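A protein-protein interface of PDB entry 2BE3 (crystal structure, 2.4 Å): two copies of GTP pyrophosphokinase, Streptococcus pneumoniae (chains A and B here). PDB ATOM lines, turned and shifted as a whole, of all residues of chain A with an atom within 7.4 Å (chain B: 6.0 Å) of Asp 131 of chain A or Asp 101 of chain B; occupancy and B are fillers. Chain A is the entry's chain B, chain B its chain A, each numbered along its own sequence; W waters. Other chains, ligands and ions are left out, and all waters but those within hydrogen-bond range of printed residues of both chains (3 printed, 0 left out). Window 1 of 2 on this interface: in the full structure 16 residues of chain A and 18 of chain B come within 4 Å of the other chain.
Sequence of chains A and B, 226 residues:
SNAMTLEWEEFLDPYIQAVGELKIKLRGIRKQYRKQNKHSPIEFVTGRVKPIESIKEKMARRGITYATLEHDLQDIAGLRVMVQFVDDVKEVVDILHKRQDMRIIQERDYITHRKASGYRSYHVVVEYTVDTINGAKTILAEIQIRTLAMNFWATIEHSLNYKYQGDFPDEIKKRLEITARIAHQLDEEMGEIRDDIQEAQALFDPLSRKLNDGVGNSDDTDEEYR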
ATOM      1  N   GLN A  17     -16.302   1.058   6.149  1.00  0.00           N
ATOM      2  CA  GLN A  17     -17.584   1.546   6.640  1.00  0.00           C
ATOM      3  C   GLN A  17     -18.122   2.766   5.838  1.00  0.00           C
ATOM      4  O   GLN A  17     -19.318   2.842   5.527  1.00  0.00           O
ATOM      5  CB  GLN A  17     -17.477   1.837   8.134  1.00  0.00           C
ATOM      6  CG  GLN A  17     -18.734   2.332   8.791  1.00  0.00           C
ATOM      7  CD  GLN A  17     -18.500   2.605  10.262  1.00  0.00           C
ATOM      8  OE1 GLN A  17     -17.492   2.174  10.830  1.00  0.00           O
ATOM      9  NE2 GLN A  17     -19.425   3.323  10.886  1.00  0.00           N
ATOM     10  N   GLU A  21     -21.695   3.248   3.779  1.00  0.00           N
ATOM     11  CA  GLU A  21     -22.702   4.237   4.135  1.00  0.00           C
ATOM     12  C   GLU A  21     -22.990   5.190   2.990  1.00  0.00           C
ATOM     13  O   GLU A  21     -24.139   5.532   2.744  1.00  0.00           O
ATOM     14  CB  GLU A  21     -22.256   5.051   5.343  1.00  0.00           C
ATOM     15  CG  GLU A  21     -22.197   4.276   6.652  1.00  0.00           C
ATOM     16  CD  GLU A  21     -21.807   5.176   7.839  1.00  0.00           C
ATOM     17  OE1 GLU A  21     -21.758   6.430   7.670  1.00  0.00           O
ATOM     18  OE2 GLU A  21     -21.557   4.632   8.939  1.00  0.00           O
ATOM     19  N   LYS A  25     -26.334   6.040   1.008  1.00  0.00           N
ATOM     20  CA  LYS A  25     -26.790   7.421   0.978  1.00  0.00           C
ATOM     21  C   LYS A  25     -26.958   7.973  -0.459  1.00  0.00           C
ATOM     22  O   LYS A  25     -27.974   8.579  -0.755  1.00  0.00           O
ATOM     23  CB  LYS A  25     -25.902   8.308   1.857  1.00  0.00           C
ATOM     24  CG  LYS A  25     -26.111   8.099   3.340  1.00  0.00           C
ATOM     25  CD  LYS A  25     -24.921   8.581   4.101  1.00  0.00           C
ATOM     26  CE  LYS A  25     -25.264   8.829   5.550  1.00  0.00           C
ATOM     27  NZ  LYS A  25     -24.331   9.828   6.130  1.00  0.00           N
ATOM     28  N   GLN A 100     -25.138  17.708   4.905  1.00  0.00           N
ATOM     29  CA  GLN A 100     -24.699  18.035   6.250  1.00  0.00           C
ATOM     30  C   GLN A 100     -23.735  16.971   6.845  1.00  0.00           C
ATOM     31  O   GLN A 100     -23.103  17.199   7.877  1.00  0.00           O
ATOM     32  CB  GLN A 100     -25.964  18.286   7.102  1.00  0.00           C
ATOM     33  CG  GLN A 100     -25.823  18.267   8.594  1.00  0.00           C
ATOM     34  CD  GLN A 100     -26.051  16.898   9.204  1.00  0.00           C
ATOM     35  OE1 GLN A 100     -25.964  16.754  10.425  1.00  0.00           O
ATOM     36  NE2 GLN A 100     -26.337  15.876   8.362  1.00  0.00           N
ATOM     37  N   TYR A 128     -15.512  12.920   5.655  1.00  0.00           N
ATOM     38  CA  TYR A 128     -16.664  12.164   6.048  1.00  0.00           C
ATOM     39  C   TYR A 128     -16.347  11.526   7.384  1.00  0.00           C
ATOM     40  O   TYR A 128     -15.237  11.055   7.595  1.00  0.00           O
ATOM     41  CB  TYR A 128     -16.963  11.104   4.994  1.00  0.00           C
ATOM     42  CG  TYR A 128     -18.266  10.389   5.235  1.00  0.00           C
ATOM     43  CD1 TYR A 128     -19.484  11.029   5.010  1.00  0.00           C
ATOM     44  CD2 TYR A 128     -18.282   9.087   5.723  1.00  0.00           C
ATOM     45  CE1 TYR A 128     -20.679  10.388   5.241  1.00  0.00           C
ATOM     46  CE2 TYR A 128     -19.485   8.417   5.964  1.00  0.00           C
ATOM     47  CZ  TYR A 128     -20.676   9.080   5.715  1.00  0.00           C
ATOM     48  OH  TYR A 128     -21.876   8.452   5.953  1.00  0.00           O
ATOM     49  N   THR A 129     -17.301  11.567   8.307  1.00  0.00           N
ATOM     50  CA  THR A 129     -17.106  11.057   9.649  1.00  0.00           C
ATOM     51  C   THR A 129     -17.976   9.847   9.811  1.00  0.00           C
ATOM     52  O   THR A 129     -19.107   9.815   9.363  1.00  0.00           O
ATOM     53  CB  THR A 129     -17.442  12.094  10.762  1.00  0.00           C
ATOM     54  OG1 THR A 129     -16.619  13.247  10.597  1.00  0.00           O
ATOM     55  CG2 THR A 129     -17.161  11.506  12.138  1.00  0.00           C
ATOM     56  N   VAL A 130     -17.409   8.847  10.455  1.00  0.00           N
ATOM     57  CA  VAL A 130     -17.989   7.527  10.582  1.00  0.00           C
ATOM     58  C   VAL A 130     -18.104   7.303  12.102  1.00  0.00           C
ATOM     59  O   VAL A 130     -17.195   7.649  12.850  1.00  0.00           O
ATOM     60  CB  VAL A 130     -17.042   6.559   9.836  1.00  0.00           C
ATOM     61  CG1 VAL A 130     -16.423   5.533  10.719  1.00  0.00           C
ATOM     62  CG2 VAL A 130     -17.656   6.007   8.526  1.00  0.00           C
ATOM     63  N   ASP A 131     -19.227   6.781  12.582  1.00  0.00           N
ATOM     64  CA  ASP A 131     -19.316   6.466  14.005  1.00  0.00           C
ATOM     65  C   ASP A 131     -18.929   5.027  14.231  1.00  0.00           C
ATOM     66  O   ASP A 131     -19.409   4.125  13.543  1.00  0.00           O
ATOM     67  CB  ASP A 131     -20.701   6.796  14.582  1.00  0.00           C
ATOM     68  CG  ASP A 131     -20.875   8.294  14.849  1.00  0.00           C
ATOM     69  OD1 ASP A 131     -20.328   8.824  15.849  1.00  0.00           O
ATOM     70  OD2 ASP A 131     -21.545   8.966  14.037  1.00  0.00           O
ATOM     71  N   THR A 132     -18.005   4.808  15.153  1.00  0.00           N
ATOM     72  CA  THR A 132     -17.627   3.444  15.502  1.00  0.00           C
ATOM     73  C   THR A 132     -17.815   3.255  16.994  1.00  0.00           C
ATOM     74  O   THR A 132     -18.023   4.230  17.748  1.00  0.00           O
ATOM     75  CB  THR A 132     -16.167   3.097  15.108  1.00  0.00           C
ATOM     76  OG1 THR A 132     -15.270   3.634  16.088  1.00  0.00           O
ATOM     77  CG2 THR A 132     -15.807   3.615  13.714  1.00  0.00           C
ATOM     78  N   ILE A 133     -17.754   2.003  17.424  1.00  0.00           N
ATOM     79  CA  ILE A 133     -17.884   1.674  18.842  1.00  0.00           C
ATOM     80  C   ILE A 133     -16.664   2.207  19.600  1.00  0.00           C
ATOM     81  O   ILE A 133     -16.662   2.277  20.825  1.00  0.00           O
ATOM     82  CB  ILE A 133     -18.051   0.138  19.072  1.00  0.00           C
ATOM     83  CG1 ILE A 133     -16.962  -0.668  18.334  1.00  0.00           C
ATOM     84  CG2 ILE A 133     -19.462  -0.318  18.641  1.00  0.00           C
ATOM     85  CD1 ILE A 133     -16.910  -2.150  18.728  1.00  0.00           C
ATOM     86  N   ASN A 134     -15.631   2.578  18.848  1.00  0.00           N
ATOM     87  CA  ASN A 134     -14.419   3.185  19.417  1.00  0.00           C
ATOM     88  C   ASN A 134     -14.363   4.686  19.197  1.00  0.00           C
ATOM     89  O   ASN A 134     -13.297   5.279  19.252  1.00  0.00           O
ATOM     90  CB  ASN A 134     -13.160   2.534  18.821  1.00  0.00           C
ATOM     91  CG  ASN A 134     -13.025   1.069  19.208  1.00  0.00           C
ATOM     92  OD1 ASN A 134     -12.601   0.239  18.395  1.00  0.00           O
ATOM     93  ND2 ASN A 134     -13.391   0.741  20.447  1.00  0.00           N
ATOM     94  N   GLY A 135     -15.515   5.291  18.936  1.00  0.00           N
ATOM     95  CA  GLY A 135     -15.577   6.707  18.624  1.00  0.00           C
ATOM     96  C   GLY A 135     -15.583   7.050  17.139  1.00  0.00           C
ATOM     97  O   GLY A 135     -15.322   6.216  16.264  1.00  0.00           O
ATOM     98  N   ALA A 136     -15.900   8.312  16.895  1.00  0.00           N
ATOM     99  CA  ALA A 136     -15.956   8.924  15.600  1.00  0.00           C
ATOM    100  C   ALA A 136     -14.579   8.970  14.961  1.00  0.00           C
ATOM    101  O   ALA A 136     -13.567   9.193  15.616  1.00  0.00           O
ATOM    102  CB  ALA A 136     -16.520  10.335  15.744  1.00  0.00           C
ATOM    103  N   LYS A 137     -14.570   8.773  13.661  1.00  0.00           N
ATOM    104  CA  LYS A 137     -13.365   8.739  12.862  1.00  0.00           C
ATOM    105  C   LYS A 137     -13.712   9.515  11.590  1.00  0.00           C
ATOM    106  O   LYS A 137     -14.692   9.215  10.910  1.00  0.00           O
ATOM    107  CB  LYS A 137     -13.007   7.274  12.549  1.00  0.00           C
ATOM    108  CG  LYS A 137     -11.663   6.762  13.115  1.00  0.00           C
ATOM    109  CD  LYS A 137     -11.682   6.247  14.582  1.00  0.00           C
ATOM    110  CE  LYS A 137     -12.128   4.768  14.726  1.00  0.00           C
ATOM    111  NZ  LYS A 137     -11.411   3.730  13.865  1.00  0.00           N
ATOM    112  N   LEU B  22     -30.915   4.332  10.430  1.00  0.00           N
ATOM    113  CA  LEU B  22     -30.655   3.966  11.812  1.00  0.00           C
ATOM    114  C   LEU B  22     -30.590   2.443  12.024  1.00  0.00           C
ATOM    115  O   LEU B  22     -29.721   1.953  12.748  1.00  0.00           O
ATOM    116  CB  LEU B  22     -31.659   4.643  12.747  1.00  0.00           C
ATOM    117  CG  LEU B  22     -31.349   6.121  13.008  1.00  0.00           C
ATOM    118  CD1 LEU B  22     -32.522   6.875  13.612  1.00  0.00           C
ATOM    119  CD2 LEU B  22     -30.130   6.187  13.897  1.00  0.00           C
ATOM    120  N   LYS B  25     -27.170   1.512  10.809  1.00  0.00           N
ATOM    121  CA  LYS B  25     -26.182   1.999  11.771  1.00  0.00           C
ATOM    122  C   LYS B  25     -26.193   1.210  13.081  1.00  0.00           C
ATOM    123  O   LYS B  25     -25.161   0.839  13.565  1.00  0.00           O
ATOM    124  CB  LYS B  25     -26.347   3.492  12.004  1.00  0.00           C
ATOM    125  CG  LYS B  25     -25.813   4.310  10.835  1.00  0.00           C
ATOM    126  CD  LYS B  25     -26.407   5.705  10.878  1.00  0.00           C
ATOM    127  CE  LYS B  25     -25.529   6.695  10.114  1.00  0.00           C
ATOM    128  NZ  LYS B  25     -26.006   8.094  10.347  1.00  0.00           N
ATOM    129  N   GLN B  32     -19.571  -4.460  14.266  1.00  0.00           N
ATOM    130  CA  GLN B  32     -18.250  -3.955  14.685  1.00  0.00           C
ATOM    131  C   GLN B  32     -17.640  -4.731  15.835  1.00  0.00           C
ATOM    132  O   GLN B  32     -16.475  -5.111  15.778  1.00  0.00           O
ATOM    133  CB  GLN B  32     -18.296  -2.472  15.038  1.00  0.00           C
ATOM    134  CG  GLN B  32     -18.081  -1.599  13.815  1.00  0.00           C
ATOM    135  CD  GLN B  32     -18.563  -0.164  13.985  1.00  0.00           C
ATOM    136  OE1 GLN B  32     -18.869   0.290  15.090  1.00  0.00           O
ATOM    137  NE2 GLN B  32     -18.635   0.556  12.879  1.00  0.00           N
ATOM    138  N   LYS B  98     -21.823   8.449  22.630  1.00  0.00           N
ATOM    139  CA  LYS B  98     -20.585   8.605  21.899  1.00  0.00           C
ATOM    140  C   LYS B  98     -20.790   9.051  20.424  1.00  0.00           C
ATOM    141  O   LYS B  98     -19.884   9.583  19.813  1.00  0.00           O
ATOM    142  CB  LYS B  98     -19.948   7.213  21.922  1.00  0.00           C
ATOM    143  CG  LYS B  98     -18.497   7.123  21.644  1.00  0.00           C
ATOM    144  CD  LYS B  98     -18.038   5.655  21.670  1.00  0.00           C
ATOM    145  CE  LYS B  98     -17.852   5.130  23.084  1.00  0.00           C
ATOM    146  NZ  LYS B  98     -17.296   3.745  23.056  1.00  0.00           N
ATOM    147  N   ARG B  99     -21.968   8.807  19.846  1.00  0.00           N
ATOM    148  CA  ARG B  99     -22.228   9.110  18.431  1.00  0.00           C
ATOM    149  C   ARG B  99     -22.434  10.596  18.121  1.00  0.00           C
ATOM    150  O   ARG B  99     -23.169  11.303  18.834  1.00  0.00           O
ATOM    151  CB  ARG B  99     -23.458   8.346  17.966  1.00  0.00           C
ATOM    152  CG  ARG B  99     -23.290   6.836  18.014  1.00  0.00           C
ATOM    153  CD  ARG B  99     -24.483   6.164  17.360  1.00  0.00           C
ATOM    154  NE  ARG B  99     -24.512   6.411  15.917  1.00  0.00           N
ATOM    155  CZ  ARG B  99     -24.003   5.584  15.002  1.00  0.00           C
ATOM    156  NH1 ARG B  99     -23.423   4.448  15.356  1.00  0.00           N
ATOM    157  NH2 ARG B  99     -24.076   5.904  13.724  1.00  0.00           N
ATOM    158  N   GLN B 100     -21.810  11.058  17.038  1.00  0.00           N
ATOM    159  CA  GLN B 100     -21.932  12.454  16.632  1.00  0.00           C
ATOM    160  C   GLN B 100     -22.994  12.628  15.547  1.00  0.00           C
ATOM    161  O   GLN B 100     -23.158  13.701  15.026  1.00  0.00           O
ATOM    162  CB  GLN B 100     -20.569  12.994  16.172  1.00  0.00           C
ATOM    163  CG  GLN B 100     -19.841  12.167  15.121  1.00  0.00           C
ATOM    164  CD  GLN B 100     -20.328  12.408  13.660  1.00  0.00           C
ATOM    165  OE1 GLN B 100     -20.205  13.533  13.122  1.00  0.00           O
ATOM    166  NE2 GLN B 100     -20.840  11.333  13.006  1.00  0.00           N
ATOM    167  N   ASP B 101     -23.706  11.558  15.187  1.00  0.00           N
ATOM    168  CA  ASP B 101     -24.755  11.657  14.169  1.00  0.00           C
ATOM    169  C   ASP B 101     -26.149  11.769  14.802  1.00  0.00           C
ATOM    170  O   ASP B 101     -27.180  11.653  14.125  1.00  0.00           O
ATOM    171  CB  ASP B 101     -24.683  10.479  13.175  1.00  0.00           C
ATOM    172  CG  ASP B 101     -24.957   9.141  13.833  1.00  0.00           C
ATOM    173  OD1 ASP B 101     -24.914   9.054  15.080  1.00  0.00           O
ATOM    174  OD2 ASP B 101     -25.204   8.154  13.104  1.00  0.00           O
ATOM    175  N   MET B 102     -26.175  11.978  16.107  1.00  0.00           N
ATOM    176  CA  MET B 102     -27.436  12.166  16.812  1.00  0.00           C
ATOM    177  C   MET B 102     -27.201  12.943  18.088  1.00  0.00           C
ATOM    178  O   MET B 102     -26.076  13.023  18.609  1.00  0.00           O
ATOM    179  CB  MET B 102     -28.089  10.811  17.138  1.00  0.00           C
ATOM    180  CG  MET B 102     -27.214   9.927  17.992  1.00  0.00           C
ATOM    181  SD  MET B 102     -27.961   8.129  18.305  1.00  0.00           S
ATOM    182  CE  MET B 102     -28.023   7.348  16.372  1.00  0.00           C
ATOM    183  N   ARG B 103     -28.278  13.503  18.604  1.00  0.00           N
ATOM    184  CA  ARG B 103     -28.217  14.199  19.863  1.00  0.00           C
ATOM    185  C   ARG B 103     -29.290  13.594  20.729  1.00  0.00           C
ATOM    186  O   ARG B 103     -30.463  13.572  20.342  1.00  0.00           O
ATOM    187  CB  ARG B 103     -28.421  15.696  19.666  1.00  0.00           C
ATOM    188  CG  ARG B 103     -28.508  16.464  20.967  1.00  0.00           C
ATOM    189  CD  ARG B 103     -28.426  17.962  20.748  1.00  0.00           C
ATOM    190  NE  ARG B 103     -29.712  18.538  20.358  1.00  0.00           N
ATOM    191  CZ  ARG B 103     -30.444  19.337  21.145  1.00  0.00           C
ATOM    192  NH1 ARG B 103     -30.008  19.644  22.375  1.00  0.00           N
ATOM    193  NH2 ARG B 103     -31.614  19.833  20.712  1.00  0.00           N
ATOM    194  N   GLU B 127     -32.408  13.446  18.482  1.00  0.00           N
ATOM    195  CA  GLU B 127     -32.522  14.244  17.280  1.00  0.00           C
ATOM    196  C   GLU B 127     -31.593  13.626  16.259  1.00  0.00           C
ATOM    197  O   GLU B 127     -30.428  13.332  16.558  1.00  0.00           O
ATOM    198  CB  GLU B 127     -32.144  15.682  17.526  1.00  0.00           C
ATOM    199  CG  GLU B 127     -33.260  16.435  18.085  1.00  0.00           C
ATOM    200  CD  GLU B 127     -32.875  17.823  18.543  1.00  0.00           C
ATOM    201  OE1 GLU B 127     -31.721  18.279  18.277  1.00  0.00           O
ATOM    202  OE2 GLU B 127     -33.758  18.457  19.170  1.00  0.00           O
ATOM    203  N   TYR B 128     -32.146  13.391  15.069  1.00  0.00           N
ATOM    204  CA  TYR B 128     -31.423  12.765  13.973  1.00  0.00           C
ATOM    205  C   TYR B 128     -31.689  13.599  12.723  1.00  0.00           C
ATOM    206  O   TYR B 128     -32.836  13.919  12.400  1.00  0.00           O
ATOM    207  CB  TYR B 128     -31.858  11.297  13.806  1.00  0.00           C
ATOM    208  CG  TYR B 128     -31.031  10.529  12.803  1.00  0.00           C
ATOM    209  CD1 TYR B 128     -29.763  10.044  13.143  1.00  0.00           C
ATOM    210  CD2 TYR B 128     -31.502  10.313  11.492  1.00  0.00           C
ATOM    211  CE1 TYR B 128     -28.989   9.354  12.224  1.00  0.00           C
ATOM    212  CE2 TYR B 128     -30.723   9.645  10.553  1.00  0.00           C
ATOM    213  CZ  TYR B 128     -29.471   9.157  10.927  1.00  0.00           C
ATOM    214  OH  TYR B 128     -28.692   8.475  10.011  1.00  0.00           O
ATOM    215  N   THR B 129     -30.619  13.985  12.042  1.00  0.00           N
ATOM    216  CA  THR B 129     -30.729  14.758  10.805  1.00  0.00           C
ATOM    217  C   THR B 129     -30.508  13.867   9.584  1.00  0.00           C
ATOM    218  O   THR B 129     -29.517  13.139   9.500  1.00  0.00           O
ATOM    219  CB  THR B 129     -29.730  15.924  10.814  1.00  0.00           C
ATOM    220  OG1 THR B 129     -30.060  16.735  11.932  1.00  0.00           O
ATOM    221  CG2 THR B 129     -29.830  16.795   9.510  1.00  0.00           C
HETATM  222  O   HOH W   1     -25.678  10.671   8.551  1.00  0.00           O
HETATM  223  O   HOH W   2     -20.902   1.778  15.312  1.00  0.00           O
HETATM  224  O   HOH W   3     -22.550   8.152  11.627  1.00  0.00           O
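OE1 of Gln 32 of chain B lies within hydrogen-bond range of N of Ile 133 of chain A. NH2 of Arg 99 of chain B lies within salt-bridge range of OD2 of Asp 131 of chain A (3.98 Å). The backbone carbonyl oxygen (O) of Ile 133 of chain A lies within hydrogen-bond range of the side-chain amino group (NZ) of Lys 98 of chain B (2.7 Å). NE2 of Gln 100 of chain B sits at hydrogen-bond distance from OD2 of Asp 131 of chain A, 2.7 Å away. The side-chain amide nitrogen (NE2) of Gln 32 of chain B sits at hydrogen-bond distance from the side-chain amide oxygen (OE1) of Gln 17 of chain A, 2.9 Å away.
The side-chain carboxylate of Glu 21 of chain A is in hydrogen-bond range of the side-chain amide nitrogen of Gln 17 of chain A (3.2 Å). The backbone carbonyl oxygen of Asp 131 of chain A is in hydrogen-bond range of the side-chain amide nitrogen of Gln 17 of chain A (2.8 Å). OG1 of Thr 132 of chain A is in hydrogen-bond range of O of Gly 135 of chain A (2.6 Å). N of Asn 134 of chain A lies close to OG1 of Thr 132 of chain A, at 3.0 Å. OD2 of Asp 101 of chain B lies within salt-bridge range of NZ of Lys 25 of chain B (2.9 Å). The guanidinium group (NH2) of Arg 99 of chain B lies within salt-bridge range of the side-chain carboxylate (OD2) of Asp 101 of chain B, at 2.6 Å.
Among the printed residues, pairs that only touch across the chains: Gln 100 of chain A with Thr 129 of chain B (3.8 Å), Thr 129 of chain A with Gln 100 of chain B (3.6 Å), Asp 131 of chain A with Gln 32 of chain B (3.7 Å), Asp 131 of chain A with Asp 101 of chain B (3.4 Å), Thr 132 of chain A with Gln 32 of chain B (3.4 Å), Gly 135 of chain A with Lys 98 of chain B (3.7 Å) and Ala 136 of chain A with Gln 100 of chain B (3.8 Å).
Of the printed residues of chain B, Asp 131 of chain A touches Gln 32 (3.7 Å), Arg 99 (3.2 Å), Gln 100 (2.7 Å) and Asp 101 (3.4 Å). Asp 101 of chain B touches one residue of chain A. Printed residues of chain A within 4 Å of Gln 100 of chain B: Thr 129, Asp 131 and Ala 136. Printed residues of chain B within 4 Å of Ala 136 of chain A: Gln 100 (3.8 Å). Printed residues of chain A within 4 Å of Thr 129 of chain B: Gln 100. Of the printed residues of chain B, Ile 133 of chain A touches Gln 32 (3.1 Å) and Lys 98 (2.7 Å). Tyr 128 of chain B touches none of the printed residues of chain A. The nearest printed residue of chain A that does not touch Asp 101 of chain B is Gln 100 of chain A (6.4 Å).
Hydrophobic or aromatic side chains of chain A that line the printed part of chain B: Ile 133 and Ala 136. Among the printed residues, 12 pairs touch across the chains.
Gln 100 of chain A touches Thr 129 of chain B, and with the chains exchanged Thr 129 of chain A touches Gln 100 of chain B. Of the 12 pairs that touch across the chains among the printed residues, 2 have their exchanged pair printed and touching as well.
Water W2 bridges the side-chain amide oxygen of Gln 32 of chain B (2.5 Å) and the backbone carbonyl oxygen of Asp 131 of chain A (3.3 Å). Water W3 lies within hydrogen-bond range of OD2 of Asp 131 of chain A (2.7 Å), OD2 of Asp 101 of chain B (3.0 Å) and NH2 of Arg 99 of chain B (3.4 Å). Water W1 bridges NZ of Lys 25 of chain A (2.9 Å) and NZ of Lys 25 of chain B (3.2 Å).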
